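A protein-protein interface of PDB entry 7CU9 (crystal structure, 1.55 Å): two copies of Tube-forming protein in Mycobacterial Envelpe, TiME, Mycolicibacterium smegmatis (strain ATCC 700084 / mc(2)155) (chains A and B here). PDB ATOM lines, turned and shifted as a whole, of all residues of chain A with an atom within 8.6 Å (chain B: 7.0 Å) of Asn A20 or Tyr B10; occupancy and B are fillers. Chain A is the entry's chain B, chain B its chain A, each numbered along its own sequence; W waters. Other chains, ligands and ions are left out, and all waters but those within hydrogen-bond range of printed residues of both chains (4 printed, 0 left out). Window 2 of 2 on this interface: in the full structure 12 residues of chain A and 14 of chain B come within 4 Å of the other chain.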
ATOM      1  N   PRO A  14       9.053   0.225 -18.519  1.00  0.00           N
ATOM      2  CA  PRO A  14       8.754   1.540 -17.958  1.00  0.00           C
ATOM      3  C   PRO A  14       8.842   1.527 -16.425  1.00  0.00           C
ATOM      4  O   PRO A  14       8.910   0.455 -15.848  1.00  0.00           O
ATOM      5  CB  PRO A  14       7.325   1.799 -18.454  1.00  0.00           C
ATOM      6  CG  PRO A  14       6.718   0.425 -18.535  1.00  0.00           C
ATOM      7  CD  PRO A  14       7.851  -0.468 -19.004  1.00  0.00           C
ATOM      8  N   LYS A  15       8.845   2.712 -15.809  1.00  0.00           N
ATOM      9  CA  LYS A  15       9.084   2.873 -14.348  1.00  0.00           C
ATOM     10  C   LYS A  15       8.099   2.012 -13.540  1.00  0.00           C
ATOM     11  O   LYS A  15       8.528   1.453 -12.518  1.00  0.00           O
ATOM     12  CB  LYS A  15       9.044   4.348 -13.941  1.00  0.00           C
ATOM     13  CG  LYS A  15       7.766   5.109 -14.259  1.00  0.00           C
ATOM     14  CD  LYS A  15       7.833   6.538 -13.770  1.00  0.00           C
ATOM     15  CE  LYS A  15       6.576   7.331 -14.052  1.00  0.00           C
ATOM     16  NZ  LYS A  15       6.803   8.780 -13.837  1.00  0.00           N
ATOM     17  N   GLY A  16       6.836   1.895 -13.967  1.00  0.00           N
ATOM     18  CA  GLY A  16       5.829   1.058 -13.282  1.00  0.00           C
ATOM     19  C   GLY A  16       6.271  -0.394 -13.186  1.00  0.00           C
ATOM     20  O   GLY A  16       6.162  -0.992 -12.104  1.00  0.00           O
ATOM     21  N   SER A  17       6.767  -0.953 -14.288  1.00  0.00           N
ATOM     22  CA  SER A  17       7.275  -2.342 -14.370  1.00  0.00           C
ATOM     23  C   SER A  17       8.555  -2.467 -13.541  1.00  0.00           C
ATOM     24  O   SER A  17       8.699  -3.466 -12.833  1.00  0.00           O
ATOM     25  CB  SER A  17       7.491  -2.746 -15.799  1.00  0.00           C
ATOM     26  OG  SER A  17       6.248  -2.783 -16.488  1.00  0.00           O
ATOM     27  N   VAL A  18       9.448  -1.482 -13.624  1.00  0.00           N
ATOM     28  CA  VAL A  18      10.716  -1.477 -12.836  1.00  0.00           C
ATOM     29  C   VAL A  18      10.360  -1.503 -11.344  1.00  0.00           C
ATOM     30  O   VAL A  18      10.962  -2.300 -10.608  1.00  0.00           O
ATOM     31  CB  VAL A  18      11.619  -0.285 -13.195  1.00  0.00           C
ATOM     32  CG1 VAL A  18      12.807  -0.185 -12.252  1.00  0.00           C
ATOM     33  CG2 VAL A  18      12.093  -0.365 -14.640  1.00  0.00           C
ATOM     34  N   SER A  19       9.393  -0.688 -10.921  1.00  0.00           N
ATOM     35  CA  SER A  19       8.918  -0.644  -9.513  1.00  0.00           C
ATOM     36  C   SER A  19       8.440  -2.037  -9.077  1.00  0.00           C
ATOM     37  O   SER A  19       8.802  -2.470  -7.968  1.00  0.00           O
ATOM     38  CB  SER A  19       7.843   0.397  -9.323  1.00  0.00           C
ATOM     39  OG  SER A  19       7.295   0.308  -8.013  1.00  0.00           O
ATOM     40  N   ASN A  20       7.653  -2.717  -9.916  1.00  0.00           N
ATOM     41  CA  ASN A  20       7.122  -4.075  -9.639  1.00  0.00           C
ATOM     42  C   ASN A  20       8.269  -5.080  -9.497  1.00  0.00           C
ATOM     43  O   ASN A  20       8.116  -6.038  -8.720  1.00  0.00           O
ATOM     44  CB  ASN A  20       6.141  -4.534 -10.718  1.00  0.00           C
ATOM     45  CG  ASN A  20       4.820  -3.801 -10.644  1.00  0.00           C
ATOM     46  OD1 ASN A  20       4.510  -3.166  -9.635  1.00  0.00           O
ATOM     47  ND2 ASN A  20       4.036  -3.886 -11.704  1.00  0.00           N
ATOM     48  N   ILE A  21       9.364  -4.889 -10.238  1.00  0.00           N
ATOM     49  CA  ILE A  21      10.510  -5.843 -10.262  1.00  0.00           C
ATOM     50  C   ILE A  21      11.402  -5.633  -9.030  1.00  0.00           C
ATOM     51  O   ILE A  21      11.799  -6.644  -8.432  1.00  0.00           O
ATOM     52  CB  ILE A  21      11.286  -5.717 -11.586  1.00  0.00           C
ATOM     53  CG1 ILE A  21      10.439  -6.228 -12.752  1.00  0.00           C
ATOM     54  CG2 ILE A  21      12.630  -6.427 -11.507  1.00  0.00           C
ATOM     55  CD1 ILE A  21      10.957  -5.824 -14.106  1.00  0.00           C
ATOM     56  N   VAL A  22      11.750  -4.392  -8.684  1.00  0.00           N
ATOM     57  CA  VAL A  22      12.687  -4.112  -7.550  1.00  0.00           C
ATOM     58  C   VAL A  22      11.931  -4.142  -6.217  1.00  0.00           C
ATOM     59  O   VAL A  22      12.605  -4.261  -5.175  1.00  0.00           O
ATOM     60  CB  VAL A  22      13.466  -2.792  -7.724  1.00  0.00           C
ATOM     61  CG1 VAL A  22      14.301  -2.807  -8.992  1.00  0.00           C
ATOM     62  CG2 VAL A  22      12.583  -1.559  -7.669  1.00  0.00           C
ATOM     63  N   GLY A  23      10.600  -4.034  -6.236  1.00  0.00           N
ATOM     64  CA  GLY A  23       9.766  -4.000  -5.017  1.00  0.00           C
ATOM     65  C   GLY A  23       9.975  -2.726  -4.221  1.00  0.00           C
ATOM     66  O   GLY A  23      10.168  -2.808  -2.991  1.00  0.00           O
ATOM     67  N   ALA A  24       9.975  -1.579  -4.898  1.00  0.00           N
ATOM     68  CA  ALA A  24      10.106  -0.243  -4.280  1.00  0.00           C
ATOM     69  C   ALA A  24       9.530   0.804  -5.224  1.00  0.00           C
ATOM     70  O   ALA A  24       9.440   0.574  -6.432  1.00  0.00           O
ATOM     71  CB  ALA A  24      11.552   0.043  -3.955  1.00  0.00           C
ATOM     72  N   PRO A  25       9.125   1.984  -4.708  1.00  0.00           N
ATOM     73  CA  PRO A  25       8.626   3.057  -5.565  1.00  0.00           C
ATOM     74  C   PRO A  25       9.698   3.519  -6.564  1.00  0.00           C
ATOM     75  O   PRO A  25      10.844   3.679  -6.188  1.00  0.00           O
ATOM     76  CB  PRO A  25       8.259   4.174  -4.574  1.00  0.00           C
ATOM     77  CG  PRO A  25       8.046   3.443  -3.269  1.00  0.00           C
ATOM     78  CD  PRO A  25       9.078   2.338  -3.280  1.00  0.00           C
ATOM     79  N   ILE A  26       9.299   3.674  -7.825  1.00  0.00           N
ATOM     80  CA  ILE A  26      10.144   4.232  -8.918  1.00  0.00           C
ATOM     81  C   ILE A  26       9.285   5.266  -9.645  1.00  0.00           C
ATOM     82  O   ILE A  26       8.493   4.860 -10.512  1.00  0.00           O
ATOM     83  CB  ILE A  26      10.637   3.114  -9.863  1.00  0.00           C
ATOM     84  CG1 ILE A  26      11.376   1.996  -9.124  1.00  0.00           C
ATOM     85  CG2 ILE A  26      11.482   3.693 -10.985  1.00  0.00           C
ATOM     86  CD1 ILE A  26      12.745   2.376  -8.605  1.00  0.00           C
ATOM     87  N   ALA A 176      16.919  -8.683  -8.712  1.00  0.00           N
ATOM     88  CA  ALA A 176      16.090  -7.746  -9.505  1.00  0.00           C
ATOM     89  C   ALA A 176      16.675  -7.582 -10.912  1.00  0.00           C
ATOM     90  O   ALA A 176      15.898  -7.583 -11.879  1.00  0.00           O
ATOM     91  CB  ALA A 176      15.965  -6.415  -8.812  1.00  0.00           C
ATOM     92  N   VAL A 179      15.664 -10.590 -12.933  1.00  0.00           N
ATOM     93  CA  VAL A 179      14.217 -10.548 -13.297  1.00  0.00           C
ATOM     94  C   VAL A 179      14.042  -9.540 -14.441  1.00  0.00           C
ATOM     95  O   VAL A 179      13.345  -9.857 -15.420  1.00  0.00           O
ATOM     96  CB  VAL A 179      13.323 -10.195 -12.093  1.00  0.00           C
ATOM     97  CG1 VAL A 179      11.898  -9.910 -12.531  1.00  0.00           C
ATOM     98  CG2 VAL A 179      13.344 -11.289 -11.038  1.00  0.00           C
ATOM     99  N   ASP B   4      10.651 -13.677  -5.696  1.00  0.00           N
ATOM    100  CA  ASP B   4      11.299 -12.544  -6.402  1.00  0.00           C
ATOM    101  C   ASP B   4      11.224 -11.322  -5.491  1.00  0.00           C
ATOM    102  O   ASP B   4      10.335 -11.227  -4.644  1.00  0.00           O
ATOM    103  CB  ASP B   4      10.631 -12.286  -7.749  1.00  0.00           C
ATOM    104  CG  ASP B   4      10.827 -13.401  -8.760  1.00  0.00           C
ATOM    105  OD1 ASP B   4      11.872 -14.069  -8.712  1.00  0.00           O
ATOM    106  OD2 ASP B   4       9.918 -13.590  -9.583  1.00  0.00           O
ATOM    107  N   PRO B   5      12.146 -10.344  -5.629  1.00  0.00           N
ATOM    108  CA  PRO B   5      12.133  -9.159  -4.771  1.00  0.00           C
ATOM    109  C   PRO B   5      10.821  -8.361  -4.833  1.00  0.00           C
ATOM    110  O   PRO B   5      10.465  -7.704  -3.852  1.00  0.00           O
ATOM    111  CB  PRO B   5      13.293  -8.277  -5.264  1.00  0.00           C
ATOM    112  CG  PRO B   5      13.974  -9.038  -6.386  1.00  0.00           C
ATOM    113  CD  PRO B   5      13.287 -10.375  -6.554  1.00  0.00           C
ATOM    114  N   GLY B   6      10.114  -8.434  -5.963  1.00  0.00           N
ATOM    115  CA  GLY B   6       8.870  -7.680  -6.187  1.00  0.00           C
ATOM    116  C   GLY B   6       7.768  -8.039  -5.201  1.00  0.00           C
ATOM    117  O   GLY B   6       6.816  -7.247  -5.088  1.00  0.00           O
ATOM    118  N   VAL B   7       7.844  -9.186  -4.523  1.00  0.00           N
ATOM    119  CA  VAL B   7       6.698  -9.654  -3.682  1.00  0.00           C
ATOM    120  C   VAL B   7       6.444  -8.655  -2.548  1.00  0.00           C
ATOM    121  O   VAL B   7       5.313  -8.639  -2.045  1.00  0.00           O
ATOM    122  CB  VAL B   7       6.872 -11.085  -3.138  1.00  0.00           C
ATOM    123  CG1 VAL B   7       6.989 -12.098  -4.264  1.00  0.00           C
ATOM    124  CG2 VAL B   7       8.022 -11.209  -2.152  1.00  0.00           C
ATOM    125  N   VAL B   8       7.434  -7.852  -2.144  1.00  0.00           N
ATOM    126  CA  VAL B   8       7.260  -6.917  -0.988  1.00  0.00           C
ATOM    127  C   VAL B   8       6.155  -5.899  -1.304  1.00  0.00           C
ATOM    128  O   VAL B   8       5.516  -5.423  -0.345  1.00  0.00           O
ATOM    129  CB  VAL B   8       8.569  -6.219  -0.570  1.00  0.00           C
ATOM    130  CG1 VAL B   8       9.613  -7.210  -0.087  1.00  0.00           C
ATOM    131  CG2 VAL B   8       9.135  -5.337  -1.663  1.00  0.00           C
ATOM    132  N   SER B   9       5.926  -5.592  -2.583  1.00  0.00           N
ATOM    133  CA  SER B   9       4.907  -4.610  -3.045  1.00  0.00           C
ATOM    134  C   SER B   9       3.481  -5.135  -2.831  1.00  0.00           C
ATOM    135  O   SER B   9       2.542  -4.308  -2.928  1.00  0.00           O
ATOM    136  CB  SER B   9       5.103  -4.242  -4.487  1.00  0.00           C
ATOM    137  OG  SER B   9       6.366  -3.624  -4.698  1.00  0.00           O
ATOM    138  N   TYR B  10       3.346  -6.449  -2.585  1.00  0.00           N
ATOM    139  CA  TYR B  10       2.067  -7.208  -2.483  1.00  0.00           C
ATOM    140  C   TYR B  10       1.873  -7.823  -1.089  1.00  0.00           C
ATOM    141  O   TYR B  10       0.710  -8.024  -0.689  1.00  0.00           O
ATOM    142  CB  TYR B  10       2.033  -8.327  -3.528  1.00  0.00           C
ATOM    143  CG  TYR B  10       2.159  -7.851  -4.953  1.00  0.00           C
ATOM    144  CD1 TYR B  10       3.400  -7.584  -5.506  1.00  0.00           C
ATOM    145  CD2 TYR B  10       1.040  -7.661  -5.749  1.00  0.00           C
ATOM    146  CE1 TYR B  10       3.531  -7.140  -6.810  1.00  0.00           C
ATOM    147  CE2 TYR B  10       1.154  -7.219  -7.058  1.00  0.00           C
ATOM    148  CZ  TYR B  10       2.403  -6.957  -7.590  1.00  0.00           C
ATOM    149  OH  TYR B  10       2.540  -6.521  -8.877  1.00  0.00           O
ATOM    150  N   ALA B  11       2.963  -8.107  -0.368  1.00  0.00           N
ATOM    151  CA  ALA B  11       2.957  -8.913   0.876  1.00  0.00           C
ATOM    152  C   ALA B  11       2.530  -8.055   2.074  1.00  0.00           C
ATOM    153  O   ALA B  11       2.173  -8.634   3.110  1.00  0.00           O
ATOM    154  CB  ALA B  11       4.309  -9.540   1.108  1.00  0.00           C
ATOM    155  N   VAL B  12       2.571  -6.727   1.944  1.00  0.00           N
ATOM    156  CA  VAL B  12       2.167  -5.787   3.029  1.00  0.00           C
ATOM    157  C   VAL B  12       0.682  -5.467   2.845  1.00  0.00           C
ATOM    158  O   VAL B  12       0.315  -4.893   1.802  1.00  0.00           O
ATOM    159  CB  VAL B  12       3.046  -4.525   3.037  1.00  0.00           C
ATOM    160  CG1 VAL B  12       2.563  -3.519   4.074  1.00  0.00           C
ATOM    161  CG2 VAL B  12       4.505  -4.876   3.267  1.00  0.00           C
ATOM    162  N   MET B  13      -0.148  -5.852   3.813  1.00  0.00           N
ATOM    163  CA  MET B  13      -1.616  -5.672   3.743  1.00  0.00           C
ATOM    164  C   MET B  13      -1.936  -4.199   3.979  1.00  0.00           C
ATOM    165  O   MET B  13      -1.409  -3.583   4.906  1.00  0.00           O
ATOM    166  CB  MET B  13      -2.334  -6.530   4.788  1.00  0.00           C
ATOM    167  CG  MET B  13      -2.138  -8.024   4.601  1.00  0.00           C
ATOM    168  SD  MET B  13      -2.778  -8.634   3.018  1.00  0.00           S
ATOM    169  CE  MET B  13      -1.243  -8.922   2.144  1.00  0.00           C
ATOM    170  N   PRO B  14      -2.807  -3.594   3.142  1.00  0.00           N
ATOM    171  CA  PRO B  14      -3.198  -2.196   3.313  1.00  0.00           C
ATOM    172  C   PRO B  14      -4.172  -2.027   4.486  1.00  0.00           C
ATOM    173  O   PRO B  14      -4.706  -3.011   4.950  1.00  0.00           O
ATOM    174  CB  PRO B  14      -3.877  -1.878   1.975  1.00  0.00           C
ATOM    175  CG  PRO B  14      -4.492  -3.187   1.568  1.00  0.00           C
ATOM    176  CD  PRO B  14      -3.477  -4.227   1.996  1.00  0.00           C
ATOM    177  N   ALA B 183      -1.961 -14.147   5.959  1.00  0.00           N
ATOM    178  CA  ALA B 183      -2.350 -13.365   4.765  1.00  0.00           C
ATOM    179  C   ALA B 183      -1.083 -12.891   4.047  1.00  0.00           C
ATOM    180  O   ALA B 183      -1.052 -12.937   2.806  1.00  0.00           O
ATOM    181  CB  ALA B 183      -3.237 -12.214   5.158  1.00  0.00           C
ATOM    182  N   MET B 184      -0.063 -12.467   4.795  1.00  0.00           N
ATOM    183  CA  MET B 184       1.220 -11.993   4.209  1.00  0.00           C
ATOM    184  C   MET B 184       1.905 -13.169   3.505  1.00  0.00           C
ATOM    185  O   MET B 184       2.333 -13.014   2.344  1.00  0.00           O
ATOM    186  CB  MET B 184       2.133 -11.416   5.294  1.00  0.00           C
ATOM    187  CG  MET B 184       1.547 -10.193   5.973  1.00  0.00           C
ATOM    188  SD  MET B 184       2.390  -9.778   7.510  1.00  0.00           S
ATOM    189  CE  MET B 184       3.920  -9.115   6.862  1.00  0.00           C
ATOM    190  N   THR B 187       0.909 -14.466  -0.106  1.00  0.00           N
ATOM    191  CA  THR B 187       1.286 -13.637  -1.288  1.00  0.00           C
ATOM    192  C   THR B 187       2.683 -13.985  -1.825  1.00  0.00           C
ATOM    193  O   THR B 187       3.064 -13.387  -2.849  1.00  0.00           O
ATOM    194  CB  THR B 187       1.248 -12.139  -0.954  1.00  0.00           C
ATOM    195  OG1 THR B 187       2.373 -11.850  -0.123  1.00  0.00           O
ATOM    196  CG2 THR B 187      -0.043 -11.713  -0.289  1.00  0.00           C
HETATM  197  O   HOH W   1       6.986  -0.946  -3.866  1.00  0.00           O
HETATM  198  O   HOH W   2       6.528  -5.253  -6.768  1.00  0.00           O
HETATM  199  O   HOH W   3       6.111  -2.021  -6.657  1.00  0.00           O
HETATM  200  O   HOH W   4      10.897  -9.133  -8.689  1.00  0.00           O
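The backbone NH (N) of Gly B6 lies within hydrogen-bond range of the backbone carbonyl oxygen (O) of Ile A21, 3.5 Å away.
Among the printed residues, pairs that only touch across the chains: Asn A20 with Gly B6, Asn A20 with Tyr B10, Ile A21 with Pro B5, Gly A23 with Pro B5, Gly A23 with Gly B6, Gly A23 with Val B8, Gly A23 with Ser B9, Ala A176 with Pro B5 and Val A179 with Asp B4.
Of the printed residues of chain B, Ile A21 touches Pro B5 (3.8 Å) and Gly B6 (3.5 Å). Printed residues of chain B within 4 Å of Ala A176: Pro B5 (3.8 Å). Printed residues of chain B within 4 Å of Val A179: Asp B4 (3.9 Å). Printed residues of chain A within 4 Å of Asp B4: Val A179. Gly B6 touches just these residues of chain A: Asn A20 (3.1 Å), Ile A21 (3.5 Å) and Gly A23 (3.96 Å). Printed residues of chain A within 4 Å of Tyr B10: Asn A20 (3.96 Å). No residue of chain A comes within 4 Å of Ala B11. Pro B14 touches none of the printed residues of chain A. The nearest printed residue of chain B that does not touch Asn A20 is Ser B9 (5.0 Å). The nearest printed residue of chain A that does not touch Tyr B10 is Ile A21 (7.1 Å).
Of the 14 printed residues of chain B, 6 touch a printed residue of chain A. Hydrophobic or aromatic side chains of chain B that line the printed part of chain A: Pro B5, Val B8 and Tyr B10. Hydrophobic or aromatic side chains of chain A within 4 Å of the printed part of chain B: Val A179. Among the printed residues, 10 pairs touch across the chains. Among the printed residues, no Asp or Glu carboxylate lies within 4 Å of a Lys or Arg side-chain nitrogen of the other chain.
1 position is printed for both chains. Of the 10 pairs that touch across the chains among the printed residues, none has its exchanged pair printed and touching as well.
Water W3 lies within hydrogen-bond range of the side-chain hydroxyl of Ser B9 and the side-chain hydroxyl of Ser A19. Water W2 lies within hydrogen-bond range of the backbone carbonyl oxygen (O) of Gly B6, the backbone carbonyl oxygen (O) of Asn A20 and the side-chain hydroxyl (OG) of Ser B9. Water W4 lies within hydrogen-bond range of O of Ile A21 and N of Gly B6. Water W1 lies within hydrogen-bond range of the side-chain hydroxyl (OG) of Ser B9 (2.9 Å) and the backbone NH (N) of Ala A24 (3.2 Å).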
